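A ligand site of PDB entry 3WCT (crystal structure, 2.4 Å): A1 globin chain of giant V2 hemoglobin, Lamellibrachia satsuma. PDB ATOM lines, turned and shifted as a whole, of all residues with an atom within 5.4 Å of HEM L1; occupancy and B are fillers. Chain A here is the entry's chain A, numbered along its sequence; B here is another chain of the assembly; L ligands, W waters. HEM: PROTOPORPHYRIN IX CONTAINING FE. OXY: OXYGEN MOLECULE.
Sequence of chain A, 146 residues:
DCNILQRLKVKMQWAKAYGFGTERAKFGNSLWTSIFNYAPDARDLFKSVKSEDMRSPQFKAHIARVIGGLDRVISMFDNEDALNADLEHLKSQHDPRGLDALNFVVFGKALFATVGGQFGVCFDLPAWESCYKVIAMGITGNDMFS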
ATOM      1  N   TRP A  32      -0.351   3.855  35.227  1.00  0.00           N
ATOM      2  CA  TRP A  32      -0.681   4.615  34.038  1.00  0.00           C
ATOM      3  C   TRP A  32      -1.797   5.636  34.184  1.00  0.00           C
ATOM      4  O   TRP A  32      -1.846   6.612  33.445  1.00  0.00           O
ATOM      5  CB  TRP A  32      -0.951   3.660  32.874  1.00  0.00           C
ATOM      6  CG  TRP A  32       0.340   3.118  32.400  1.00  0.00           C
ATOM      7  CD1 TRP A  32       0.932   1.951  32.785  1.00  0.00           C
ATOM      8  CD2 TRP A  32       1.279   3.793  31.557  1.00  0.00           C
ATOM      9  NE1 TRP A  32       2.189   1.865  32.247  1.00  0.00           N
ATOM     10  CE2 TRP A  32       2.426   2.980  31.495  1.00  0.00           C
ATOM     11  CE3 TRP A  32       1.261   5.005  30.864  1.00  0.00           C
ATOM     12  CZ2 TRP A  32       3.565   3.345  30.755  1.00  0.00           C
ATOM     13  CZ3 TRP A  32       2.393   5.377  30.124  1.00  0.00           C
ATOM     14  CH2 TRP A  32       3.529   4.538  30.080  1.00  0.00           C
ATOM     15  N   ALA A  42       0.776  13.768  27.979  1.00  0.00           N
ATOM     16  CA  ALA A  42       1.541  12.565  27.660  1.00  0.00           C
ATOM     17  C   ALA A  42       0.663  11.463  27.074  1.00  0.00           C
ATOM     18  O   ALA A  42       1.153  10.573  26.374  1.00  0.00           O
ATOM     19  CB  ALA A  42       2.250  12.058  28.907  1.00  0.00           C
ATOM     20  N   LEU A  45       0.825  10.620  23.414  1.00  0.00           N
ATOM     21  CA  LEU A  45       2.058   9.961  22.977  1.00  0.00           C
ATOM     22  C   LEU A  45       1.901   8.449  22.770  1.00  0.00           C
ATOM     23  O   LEU A  45       2.806   7.806  22.237  1.00  0.00           O
ATOM     24  CB  LEU A  45       3.178  10.211  23.998  1.00  0.00           C
ATOM     25  CG  LEU A  45       3.401  11.667  24.402  1.00  0.00           C
ATOM     26  CD1 LEU A  45       4.370  11.748  25.573  1.00  0.00           C
ATOM     27  CD2 LEU A  45       3.941  12.453  23.205  1.00  0.00           C
ATOM     28  N   PHE A  46       0.755   7.896  23.178  1.00  0.00           N
ATOM     29  CA  PHE A  46       0.539   6.453  23.071  1.00  0.00           C
ATOM     30  C   PHE A  46      -0.612   6.016  22.193  1.00  0.00           C
ATOM     31  O   PHE A  46      -1.240   4.988  22.449  1.00  0.00           O
ATOM     32  CB  PHE A  46       0.362   5.862  24.467  1.00  0.00           C
ATOM     33  CG  PHE A  46       1.511   6.141  25.381  1.00  0.00           C
ATOM     34  CD1 PHE A  46       2.518   5.186  25.565  1.00  0.00           C
ATOM     35  CD2 PHE A  46       1.613   7.360  26.050  1.00  0.00           C
ATOM     36  CE1 PHE A  46       3.607   5.457  26.388  1.00  0.00           C
ATOM     37  CE2 PHE A  46       2.704   7.633  26.883  1.00  0.00           C
ATOM     38  CZ  PHE A  46       3.700   6.681  27.047  1.00  0.00           C
ATOM     39  N   SER A  48      -0.355   4.813  19.470  1.00  0.00           N
ATOM     40  CA  SER A  48       0.081   3.578  18.826  1.00  0.00           C
ATOM     41  C   SER A  48      -0.337   2.332  19.611  1.00  0.00           C
ATOM     42  O   SER A  48      -0.398   1.231  19.044  1.00  0.00           O
ATOM     43  CB  SER A  48       1.606   3.591  18.632  1.00  0.00           C
ATOM     44  OG  SER A  48       2.312   3.917  19.819  1.00  0.00           O
ATOM     45  N   VAL A  49      -0.634   2.496  20.904  1.00  0.00           N
ATOM     46  CA  VAL A  49      -1.107   1.383  21.744  1.00  0.00           C
ATOM     47  C   VAL A  49      -2.511   1.633  22.263  1.00  0.00           C
ATOM     48  O   VAL A  49      -2.906   1.111  23.311  1.00  0.00           O
ATOM     49  CB  VAL A  49      -0.182   1.100  22.951  1.00  0.00           C
ATOM     50  CG1 VAL A  49       1.059   0.362  22.479  1.00  0.00           C
ATOM     51  CG2 VAL A  49       0.175   2.384  23.671  1.00  0.00           C
ATOM     52  N   HIS A  62       0.458  -3.035  26.499  1.00  0.00           N
ATOM     53  CA  HIS A  62       1.517  -2.055  26.680  1.00  0.00           C
ATOM     54  C   HIS A  62       1.863  -1.925  28.169  1.00  0.00           C
ATOM     55  O   HIS A  62       3.043  -1.871  28.533  1.00  0.00           O
ATOM     56  CB  HIS A  62       1.093  -0.687  26.156  1.00  0.00           C
ATOM     57  CG  HIS A  62       2.063   0.405  26.476  1.00  0.00           C
ATOM     58  ND1 HIS A  62       3.300   0.500  25.871  1.00  0.00           N
ATOM     59  CD2 HIS A  62       2.006   1.419  27.367  1.00  0.00           C
ATOM     60  CE1 HIS A  62       3.953   1.524  26.372  1.00  0.00           C
ATOM     61  NE2 HIS A  62       3.201   2.102  27.286  1.00  0.00           N
ATOM     62  N   ARG A  65       3.787  -4.869  29.232  1.00  0.00           N
ATOM     63  CA  ARG A  65       5.174  -4.789  28.768  1.00  0.00           C
ATOM     64  C   ARG A  65       6.015  -3.822  29.610  1.00  0.00           C
ATOM     65  O   ARG A  65       7.160  -4.109  29.942  1.00  0.00           O
ATOM     66  CB  ARG A  65       5.240  -4.416  27.286  1.00  0.00           C
ATOM     67  CG  ARG A  65       4.831  -5.528  26.330  1.00  0.00           C
ATOM     68  CD  ARG A  65       5.203  -5.226  24.866  1.00  0.00           C
ATOM     69  NE  ARG A  65       4.363  -4.207  24.240  1.00  0.00           N
ATOM     70  CZ  ARG A  65       3.129  -4.420  23.786  1.00  0.00           C
ATOM     71  NH1 ARG A  65       2.570  -5.624  23.881  1.00  0.00           N
ATOM     72  NH2 ARG A  65       2.443  -3.412  23.247  1.00  0.00           N
ATOM     73  N   VAL A  66       5.452  -2.682  29.966  1.00  0.00           N
ATOM     74  CA  VAL A  66       6.183  -1.700  30.764  1.00  0.00           C
ATOM     75  C   VAL A  66       6.498  -2.138  32.207  1.00  0.00           C
ATOM     76  O   VAL A  66       7.626  -1.992  32.675  1.00  0.00           O
ATOM     77  CB  VAL A  66       5.423  -0.353  30.810  1.00  0.00           C
ATOM     78  CG1 VAL A  66       6.122   0.613  31.773  1.00  0.00           C
ATOM     79  CG2 VAL A  66       5.351   0.223  29.393  1.00  0.00           C
ATOM     80  N   GLY A  69       8.922  -4.554  32.128  1.00  0.00           N
ATOM     81  CA  GLY A  69      10.235  -3.953  31.949  1.00  0.00           C
ATOM     82  C   GLY A  69      10.796  -3.499  33.282  1.00  0.00           C
ATOM     83  O   GLY A  69      11.939  -3.789  33.605  1.00  0.00           O
ATOM     84  N   LEU A  70       9.975  -2.795  34.056  1.00  0.00           N
ATOM     85  CA  LEU A  70      10.374  -2.322  35.375  1.00  0.00           C
ATOM     86  C   LEU A  70      10.830  -3.492  36.245  1.00  0.00           C
ATOM     87  O   LEU A  70      11.843  -3.418  36.939  1.00  0.00           O
ATOM     88  CB  LEU A  70       9.202  -1.610  36.049  1.00  0.00           C
ATOM     89  CG  LEU A  70       9.041  -0.107  35.767  1.00  0.00           C
ATOM     90  CD1 LEU A  70       7.702   0.385  36.324  1.00  0.00           C
ATOM     91  CD2 LEU A  70      10.208   0.633  36.398  1.00  0.00           C
ATOM     92  N   ARG A  72      11.982  -6.617  35.330  1.00  0.00           N
ATOM     93  CA  ARG A  72      13.245  -7.258  34.935  1.00  0.00           C
ATOM     94  C   ARG A  72      14.434  -6.343  35.231  1.00  0.00           C
ATOM     95  O   ARG A  72      15.506  -6.806  35.637  1.00  0.00           O
ATOM     96  CB  ARG A  72      13.216  -7.649  33.453  1.00  0.00           C
ATOM     97  CG  ARG A  72      13.323  -6.487  32.507  1.00  0.00           C
ATOM     98  CD  ARG A  72      13.009  -6.901  31.075  1.00  0.00           C
ATOM     99  NE  ARG A  72      13.644  -5.966  30.150  1.00  0.00           N
ATOM    100  CZ  ARG A  72      13.107  -5.537  29.012  1.00  0.00           C
ATOM    101  NH1 ARG A  72      11.899  -5.939  28.648  1.00  0.00           N
ATOM    102  NH2 ARG A  72      13.785  -4.685  28.264  1.00  0.00           N
ATOM    103  N   LEU A  90      16.580  -0.924  26.240  1.00  0.00           N
ATOM    104  CA  LEU A  90      15.397  -0.103  26.412  1.00  0.00           C
ATOM    105  C   LEU A  90      15.638   1.280  25.829  1.00  0.00           C
ATOM    106  O   LEU A  90      14.706   1.947  25.402  1.00  0.00           O
ATOM    107  CB  LEU A  90      15.015   0.019  27.898  1.00  0.00           C
ATOM    108  CG  LEU A  90      14.544  -1.268  28.598  1.00  0.00           C
ATOM    109  CD1 LEU A  90      14.302  -0.972  30.060  1.00  0.00           C
ATOM    110  CD2 LEU A  90      13.277  -1.810  27.932  1.00  0.00           C
ATOM    111  N   GLN A  93      15.031   1.513  22.099  1.00  0.00           N
ATOM    112  CA  GLN A  93      13.612   1.412  21.761  1.00  0.00           C
ATOM    113  C   GLN A  93      12.870   2.738  21.944  1.00  0.00           C
ATOM    114  O   GLN A  93      11.871   2.982  21.281  1.00  0.00           O
ATOM    115  CB  GLN A  93      12.922   0.318  22.597  1.00  0.00           C
ATOM    116  CG  GLN A  93      13.400  -1.098  22.318  1.00  0.00           C
ATOM    117  CD  GLN A  93      12.951  -2.095  23.388  1.00  0.00           C
ATOM    118  OE1 GLN A  93      13.153  -1.874  24.582  1.00  0.00           O
ATOM    119  NE2 GLN A  93      12.334  -3.196  22.960  1.00  0.00           N
ATOM    120  N   HIS A  94      13.358   3.584  22.860  1.00  0.00           N
ATOM    121  CA  HIS A  94      12.707   4.874  23.096  1.00  0.00           C
ATOM    122  C   HIS A  94      13.326   6.041  22.310  1.00  0.00           C
ATOM    123  O   HIS A  94      12.621   6.990  21.975  1.00  0.00           O
ATOM    124  CB  HIS A  94      12.712   5.199  24.608  1.00  0.00           C
ATOM    125  CG  HIS A  94      11.794   4.343  25.414  1.00  0.00           C
ATOM    126  ND1 HIS A  94      12.057   3.018  25.699  1.00  0.00           N
ATOM    127  CD2 HIS A  94      10.606   4.618  26.010  1.00  0.00           C
ATOM    128  CE1 HIS A  94      11.082   2.521  26.436  1.00  0.00           C
ATOM    129  NE2 HIS A  94      10.179   3.476  26.639  1.00  0.00           N
ATOM    130  N   ARG A  97      11.789   7.787  19.197  1.00  0.00           N
ATOM    131  CA  ARG A  97      10.451   8.317  19.390  1.00  0.00           C
ATOM    132  C   ARG A  97      10.447   9.781  19.806  1.00  0.00           C
ATOM    133  O   ARG A  97       9.385  10.369  20.048  1.00  0.00           O
ATOM    134  CB  ARG A  97       9.683   7.491  20.411  1.00  0.00           C
ATOM    135  CG  ARG A  97       9.759   5.989  20.177  1.00  0.00           C
ATOM    136  CD  ARG A  97       8.644   5.273  20.897  1.00  0.00           C
ATOM    137  NE  ARG A  97       7.465   5.081  20.053  1.00  0.00           N
ATOM    138  CZ  ARG A  97       7.263   4.016  19.275  1.00  0.00           C
ATOM    139  NH1 ARG A  97       8.170   3.040  19.243  1.00  0.00           N
ATOM    140  NH2 ARG A  97       6.151   3.910  18.555  1.00  0.00           N
ATOM    141  N   LEU A  99      11.056  11.368  22.536  1.00  0.00           N
ATOM    142  CA  LEU A  99      10.292  11.592  23.760  1.00  0.00           C
ATOM    143  C   LEU A  99      10.972  12.637  24.626  1.00  0.00           C
ATOM    144  O   LEU A  99      12.193  12.614  24.791  1.00  0.00           O
ATOM    145  CB  LEU A  99      10.183  10.308  24.578  1.00  0.00           C
ATOM    146  CG  LEU A  99       9.729   9.053  23.840  1.00  0.00           C
ATOM    147  CD1 LEU A  99       9.798   7.871  24.798  1.00  0.00           C
ATOM    148  CD2 LEU A  99       8.313   9.256  23.297  1.00  0.00           C
ATOM    149  N   ASN A 103       9.093  13.747  30.833  1.00  0.00           N
ATOM    150  CA  ASN A 103       8.010  12.793  31.046  1.00  0.00           C
ATOM    151  C   ASN A 103       8.478  11.563  31.834  1.00  0.00           C
ATOM    152  O   ASN A 103       7.662  10.792  32.309  1.00  0.00           O
ATOM    153  CB  ASN A 103       7.406  12.354  29.718  1.00  0.00           C
ATOM    154  CG  ASN A 103       6.391  13.351  29.193  1.00  0.00           C
ATOM    155  OD1 ASN A 103       5.906  13.227  28.064  1.00  0.00           O
ATOM    156  ND2 ASN A 103       6.045  14.351  30.007  1.00  0.00           N
ATOM    157  N   PHE A 104       9.783  11.395  31.952  1.00  0.00           N
ATOM    158  CA  PHE A 104      10.312  10.286  32.721  1.00  0.00           C
ATOM    159  C   PHE A 104      10.344  10.666  34.184  1.00  0.00           C
ATOM    160  O   PHE A 104      10.419   9.807  35.059  1.00  0.00           O
ATOM    161  CB  PHE A 104      11.707   9.882  32.228  1.00  0.00           C
ATOM    162  CG  PHE A 104      11.692   9.032  31.001  1.00  0.00           C
ATOM    163  CD1 PHE A 104      11.776   7.646  31.105  1.00  0.00           C
ATOM    164  CD2 PHE A 104      11.520   9.608  29.739  1.00  0.00           C
ATOM    165  CE1 PHE A 104      11.689   6.839  29.957  1.00  0.00           C
ATOM    166  CE2 PHE A 104      11.435   8.817  28.597  1.00  0.00           C
ATOM    167  CZ  PHE A 104      11.526   7.425  28.701  1.00  0.00           C
ATOM    168  N   PHE A 107       6.808   9.970  35.118  1.00  0.00           N
ATOM    169  CA  PHE A 107       6.671   8.527  35.236  1.00  0.00           C
ATOM    170  C   PHE A 107       7.119   8.083  36.624  1.00  0.00           C
ATOM    171  O   PHE A 107       6.396   7.357  37.321  1.00  0.00           O
ATOM    172  CB  PHE A 107       7.496   7.835  34.145  1.00  0.00           C
ATOM    173  CG  PHE A 107       7.343   6.345  34.110  1.00  0.00           C
ATOM    174  CD1 PHE A 107       7.894   5.551  35.097  1.00  0.00           C
ATOM    175  CD2 PHE A 107       6.651   5.731  33.067  1.00  0.00           C
ATOM    176  CE1 PHE A 107       7.762   4.155  35.057  1.00  0.00           C
ATOM    177  CE2 PHE A 107       6.510   4.340  33.017  1.00  0.00           C
ATOM    178  CZ  PHE A 107       7.068   3.553  34.002  1.00  0.00           C
ATOM    179  N   TYR A 132      15.478   5.111  40.897  1.00  0.00           N
ATOM    180  CA  TYR A 132      14.670   5.272  39.704  1.00  0.00           C
ATOM    181  C   TYR A 132      15.552   6.028  38.709  1.00  0.00           C
ATOM    182  O   TYR A 132      15.628   5.665  37.544  1.00  0.00           O
ATOM    183  CB  TYR A 132      13.392   6.082  39.981  1.00  0.00           C
ATOM    184  CG  TYR A 132      12.670   6.416  38.702  1.00  0.00           C
ATOM    185  CD1 TYR A 132      12.635   7.729  38.218  1.00  0.00           C
ATOM    186  CD2 TYR A 132      12.092   5.421  37.919  1.00  0.00           C
ATOM    187  CE1 TYR A 132      12.063   8.034  37.011  1.00  0.00           C
ATOM    188  CE2 TYR A 132      11.510   5.714  36.695  1.00  0.00           C
ATOM    189  CZ  TYR A 132      11.495   7.020  36.241  1.00  0.00           C
ATOM    190  OH  TYR A 132      10.928   7.329  35.021  1.00  0.00           O
ATOM    191  N   ILE A 135      17.550   4.166  36.431  1.00  0.00           N
ATOM    192  CA  ILE A 135      16.726   3.573  35.377  1.00  0.00           C
ATOM    193  C   ILE A 135      16.394   4.564  34.252  1.00  0.00           C
ATOM    194  O   ILE A 135      16.545   4.250  33.062  1.00  0.00           O
ATOM    195  CB  ILE A 135      15.407   3.003  35.969  1.00  0.00           C
ATOM    196  CG1 ILE A 135      15.721   1.845  36.926  1.00  0.00           C
ATOM    197  CG2 ILE A 135      14.489   2.543  34.841  1.00  0.00           C
ATOM    198  CD1 ILE A 135      14.492   1.197  37.579  1.00  0.00           C
ATOM    199  N   ALA A 136      15.928   5.748  34.632  1.00  0.00           N
ATOM    200  CA  ALA A 136      15.556   6.786  33.670  1.00  0.00           C
ATOM    201  C   ALA A 136      16.764   7.280  32.878  1.00  0.00           C
ATOM    202  O   ALA A 136      16.653   7.633  31.706  1.00  0.00           O
ATOM    203  CB  ALA A 136      14.889   7.941  34.388  1.00  0.00           C
ATOM    204  N   ILE A 139      17.731   4.855  30.258  1.00  0.00           N
ATOM    205  CA  ILE A 139      16.802   4.860  29.144  1.00  0.00           C
ATOM    206  C   ILE A 139      16.861   6.165  28.363  1.00  0.00           C
ATOM    207  O   ILE A 139      16.685   6.173  27.155  1.00  0.00           O
ATOM    208  CB  ILE A 139      15.344   4.590  29.612  1.00  0.00           C
ATOM    209  CG1 ILE A 139      15.229   3.166  30.180  1.00  0.00           C
ATOM    210  CG2 ILE A 139      14.376   4.728  28.445  1.00  0.00           C
ATOM    211  CD1 ILE A 139      13.824   2.822  30.696  1.00  0.00           C
ATOM    212  N   HIS B  94       2.259  -9.071  19.505  1.00  0.00           N
ATOM    213  CA  HIS B  94       3.428  -8.196  19.584  1.00  0.00           C
ATOM    214  C   HIS B  94       4.682  -9.055  19.594  1.00  0.00           C
ATOM    215  O   HIS B  94       5.565  -8.873  18.757  1.00  0.00           O
ATOM    216  CB  HIS B  94       3.356  -7.335  20.845  1.00  0.00           C
ATOM    217  CG  HIS B  94       4.483  -6.344  20.969  1.00  0.00           C
ATOM    218  ND1 HIS B  94       5.687  -6.666  21.569  1.00  0.00           N
ATOM    219  CD2 HIS B  94       4.589  -5.055  20.579  1.00  0.00           C
ATOM    220  CE1 HIS B  94       6.482  -5.604  21.544  1.00  0.00           C
ATOM    221  NE2 HIS B  94       5.835  -4.614  20.949  1.00  0.00           N
ATOM    222  N   GLN B  98       7.995  -9.435  17.024  1.00  0.00           N
ATOM    223  CA  GLN B  98       9.405  -9.300  17.388  1.00  0.00           C
ATOM    224  C   GLN B  98      10.264 -10.494  16.924  1.00  0.00           C
ATOM    225  O   GLN B  98      11.501 -10.445  16.986  1.00  0.00           O
ATOM    226  CB  GLN B  98       9.561  -9.121  18.903  1.00  0.00           C
ATOM    227  CG  GLN B  98       9.017  -7.813  19.468  1.00  0.00           C
ATOM    228  CD  GLN B  98       9.139  -7.742  20.993  1.00  0.00           C
ATOM    229  OE1 GLN B  98       8.708  -8.656  21.707  1.00  0.00           O
ATOM    230  NE2 GLN B  98       9.722  -6.647  21.502  1.00  0.00           N
HETATM  231  CHA HEM L   1       7.347   1.077  24.896  1.00  0.00           C
HETATM  232  CHB HEM L   1       9.477   0.376  29.090  1.00  0.00           C
HETATM  233  CHC HEM L   1       8.896   5.027  30.234  1.00  0.00           C
HETATM  234  CHD HEM L   1       6.980   5.745  25.879  1.00  0.00           C
HETATM  235  C1A HEM L   1       7.969   0.461  25.955  1.00  0.00           C
HETATM  236  C2A HEM L   1       8.213  -0.918  25.995  1.00  0.00           C
HETATM  237  C3A HEM L   1       8.830  -1.118  27.171  1.00  0.00           C
HETATM  238  C4A HEM L   1       8.960   0.145  27.876  1.00  0.00           C
HETATM  239  CMA HEM L   1       9.330  -2.465  27.717  1.00  0.00           C
HETATM  240  CAA HEM L   1       7.852  -1.952  24.950  1.00  0.00           C
HETATM  241  CBA HEM L   1       8.968  -2.166  23.947  1.00  0.00           C
HETATM  242  CGA HEM L   1       8.646  -3.188  22.849  1.00  0.00           C
HETATM  243  O1A HEM L   1       8.509  -2.806  21.655  1.00  0.00           O
HETATM  244  O2A HEM L   1       8.525  -4.335  23.159  1.00  0.00           O
HETATM  245  C1B HEM L   1       9.531   1.589  29.811  1.00  0.00           C
HETATM  246  C2B HEM L   1      10.064   1.724  31.148  1.00  0.00           C
HETATM  247  C3B HEM L   1       9.875   3.124  31.468  1.00  0.00           C
HETATM  248  C4B HEM L   1       9.274   3.688  30.333  1.00  0.00           C
HETATM  249  CMB HEM L   1      10.645   0.641  31.995  1.00  0.00           C
HETATM  250  CAB HEM L   1      10.233   3.725  32.755  1.00  0.00           C
HETATM  251  CBB HEM L   1      11.443   4.070  33.122  1.00  0.00           C
HETATM  252  C1C HEM L   1       8.309   5.621  29.131  1.00  0.00           C
HETATM  253  C2C HEM L   1       7.938   7.054  29.104  1.00  0.00           C
HETATM  254  C3C HEM L   1       7.387   7.307  27.820  1.00  0.00           C
HETATM  255  C4C HEM L   1       7.441   5.948  27.142  1.00  0.00           C
HETATM  256  CMC HEM L   1       8.126   8.040  30.256  1.00  0.00           C
HETATM  257  CAC HEM L   1       6.930   8.469  27.317  1.00  0.00           C
HETATM  258  CBC HEM L   1       6.040   9.366  27.550  1.00  0.00           C
HETATM  259  C1D HEM L   1       6.923   4.545  25.218  1.00  0.00           C
HETATM  260  C2D HEM L   1       6.325   4.370  23.841  1.00  0.00           C
HETATM  261  C3D HEM L   1       6.438   3.022  23.576  1.00  0.00           C
HETATM  262  C4D HEM L   1       7.078   2.413  24.765  1.00  0.00           C
HETATM  263  CMD HEM L   1       5.730   5.497  22.997  1.00  0.00           C
HETATM  264  CAD HEM L   1       5.998   2.292  22.312  1.00  0.00           C
HETATM  265  CBD HEM L   1       4.631   1.705  22.395  1.00  0.00           C
HETATM  266  CGD HEM L   1       4.237   0.980  21.183  1.00  0.00           C
HETATM  267  O1D HEM L   1       3.599   1.583  20.266  1.00  0.00           O
HETATM  268  O2D HEM L   1       4.536  -0.228  21.060  1.00  0.00           O
HETATM  269  NA  HEM L   1       8.430   1.124  27.104  1.00  0.00           N
HETATM  270  NB  HEM L   1       9.072   2.733  29.291  1.00  0.00           N
HETATM  271  NC  HEM L   1       7.988   5.001  27.924  1.00  0.00           N
HETATM  272  ND  HEM L   1       7.369   3.372  25.705  1.00  0.00           N
HETATM  273 FE   HEM L   1       8.262   3.066  27.487  1.00  0.00          FE
HETATM  274  O1  OXY L   2       6.636   2.771  28.171  1.00  0.00           O
HETATM  275  O2  OXY L   2       5.586   3.422  28.136  1.00  0.00           O
HETATM  276  CHA HEM L   3      14.135 -11.951  21.147  1.00  0.00           C
HETATM  277  CHB HEM L   3      10.881 -13.992  23.920  1.00  0.00           C
HETATM  278  CHC HEM L   3      11.588 -18.228  21.753  1.00  0.00           C
HETATM  279  CHD HEM L   3      14.702 -16.089  18.818  1.00  0.00           C
HETATM  280  C1A HEM L   3      13.183 -12.116  22.108  1.00  0.00           C
HETATM  281  C2A HEM L   3      12.770 -11.112  22.987  1.00  0.00           C
HETATM  282  C3A HEM L   3      11.826 -11.678  23.765  1.00  0.00           C
HETATM  283  C4A HEM L   3      11.671 -13.062  23.383  1.00  0.00           C
HETATM  284  CMA HEM L   3      11.024 -11.019  24.900  1.00  0.00           C
HETATM  285  CAA HEM L   3      13.264  -9.684  23.074  1.00  0.00           C
HETATM  286  CBA HEM L   3      12.449  -8.774  22.207  1.00  0.00           C
HETATM  287  CGA HEM L   3      12.885  -7.307  22.182  1.00  0.00           C
HETATM  288  O1A HEM L   3      13.236  -6.788  21.091  1.00  0.00           O
HETATM  289  O2A HEM L   3      12.889  -6.704  23.204  1.00  0.00           O
HETATM  290  C1B HEM L   3      10.777 -15.366  23.610  1.00  0.00           C
HETATM  291  C2B HEM L   3       9.935 -16.303  24.325  1.00  0.00           C
HETATM  292  C3B HEM L   3      10.190 -17.567  23.681  1.00  0.00           C
HETATM  293  C4B HEM L   3      11.105 -17.283  22.638  1.00  0.00           C
HETATM  294  CMB HEM L   3       9.040 -16.015  25.467  1.00  0.00           C
HETATM  295  CAB HEM L   3       9.592 -18.819  24.096  1.00  0.00           C
HETATM  296  CBB HEM L   3       8.388 -19.217  23.719  1.00  0.00           C
HETATM  297  C1C HEM L   3      12.495 -17.995  20.744  1.00  0.00           C
HETATM  298  C2C HEM L   3      12.966 -19.053  19.834  1.00  0.00           C
HETATM  299  C3C HEM L   3      13.876 -18.453  18.951  1.00  0.00           C
HETATM  300  C4C HEM L   3      13.922 -17.008  19.403  1.00  0.00           C
HETATM  301  CMC HEM L   3      12.530 -20.520  19.859  1.00  0.00           C
HETATM  302  CAC HEM L   3      14.572 -19.048  17.937  1.00  0.00           C
HETATM  303  CBC HEM L   3      15.733 -19.561  17.722  1.00  0.00           C
HETATM  304  C1D HEM L   3      14.828 -14.765  19.198  1.00  0.00           C
HETATM  305  C2D HEM L   3      15.789 -13.817  18.541  1.00  0.00           C
HETATM  306  C3D HEM L   3      15.621 -12.635  19.228  1.00  0.00           C
HETATM  307  C4D HEM L   3      14.580 -12.876  20.255  1.00  0.00           C
HETATM  308  CMD HEM L   3      16.725 -14.179  17.386  1.00  0.00           C
HETATM  309  CAD HEM L   3      16.364 -11.342  19.005  1.00  0.00           C
HETATM  310  CBD HEM L   3      17.635 -11.301  19.802  1.00  0.00           C
HETATM  311  CGD HEM L   3      18.382 -10.062  19.601  1.00  0.00           C
HETATM  312  O1D HEM L   3      17.998  -9.005  20.181  1.00  0.00           O
HETATM  313  O2D HEM L   3      19.385 -10.070  18.866  1.00  0.00           O
HETATM  314  NA  HEM L   3      12.505 -13.326  22.332  1.00  0.00           N
HETATM  315  NB  HEM L   3      11.477 -15.912  22.615  1.00  0.00           N
HETATM  316  NC  HEM L   3      13.098 -16.778  20.429  1.00  0.00           N
HETATM  317  ND  HEM L   3      14.150 -14.165  20.197  1.00  0.00           N
HETATM  318 FE   HEM L   3      12.776 -15.028  21.364  1.00  0.00          FE
HETATM  319  O   HOH W   1       3.313  -0.006  17.870  1.00  0.00           O
HETATM  320  O   HOH W   2       4.615  -1.312  24.226  1.00  0.00           O
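An oxygen (O1) of OXY L2 is bound to an iron atom (FE) of HEM L1 (1.8 Å).
Water W2 lies within hydrogen-bond range of ND1 of His 62 (2.8 Å), NE of Arg 65 (2.9 Å) and O2D of HEM L1 (3.3 Å).
The backbone carbonyl oxygen (O) of Phe 104 lies within hydrogen-bond range of the side-chain hydroxyl (OH) of Tyr 132 (2.5 Å).
The backbone carbonyl oxygen (O) of Leu 90 lies within hydrogen-bond range of a ring nitrogen (ND1) of His 94 of chain A, at 2.9 Å.
A ring nitrogen (NE2) of His 94 of chain B lies within hydrogen-bond range of an oxygen (O1A) of HEM L1, 3.3 Å away.
The side-chain hydroxyl (OG) of Ser 48 sits at hydrogen-bond distance from an oxygen (O1D) of HEM L1, 2.7 Å away.
The guanidinium group (NH2) of Arg 97 is in salt-bridge range of an oxygen (O1D) of HEM L1.
The side-chain amide nitrogen of Gln 98 of chain B lies within hydrogen-bond range of an oxygen (O2A) of HEM L1 (3.1 Å).
NE2 of His 62 is in hydrogen-bond range of O2 of OXY L2 (2.9 Å).
A ring nitrogen (NE2) of His 94 of chain A is bound to an iron atom (FE) of HEM L1.
Merely in contact with HEM L1: Leu 45, Phe 46, Val 49, His 62, Arg 65, Val 66, Gln 93, Leu 99, Asn 103, Phe 104, Phe 107, Tyr 132, Ile 135 and Ile 139.
Hydrophobic or aromatic side chains that line HEM L1: Leu 45, Phe 46, Val 49, His 62, Val 66, His 94 of chain A, Leu 99, Phe 104, Phe 107, Tyr 132, Ile 135, Ile 139 and His 94 of chain B.
19 residues have an atom within 4 Å of HEM L1: Leu 45, Phe 46, Ser 48, Val 49, His 62, Arg 65, Val 66, Gln 93, His 94 of chain A, Arg 97, Leu 99, Asn 103, Phe 104, Phe 107, Tyr 132, Ile 135, Ile 139, His 94 of chain B and Gln 98 of chain B.
The nearest printed residue that does not touch HEM L1 is Leu 90 (4.01 Å).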
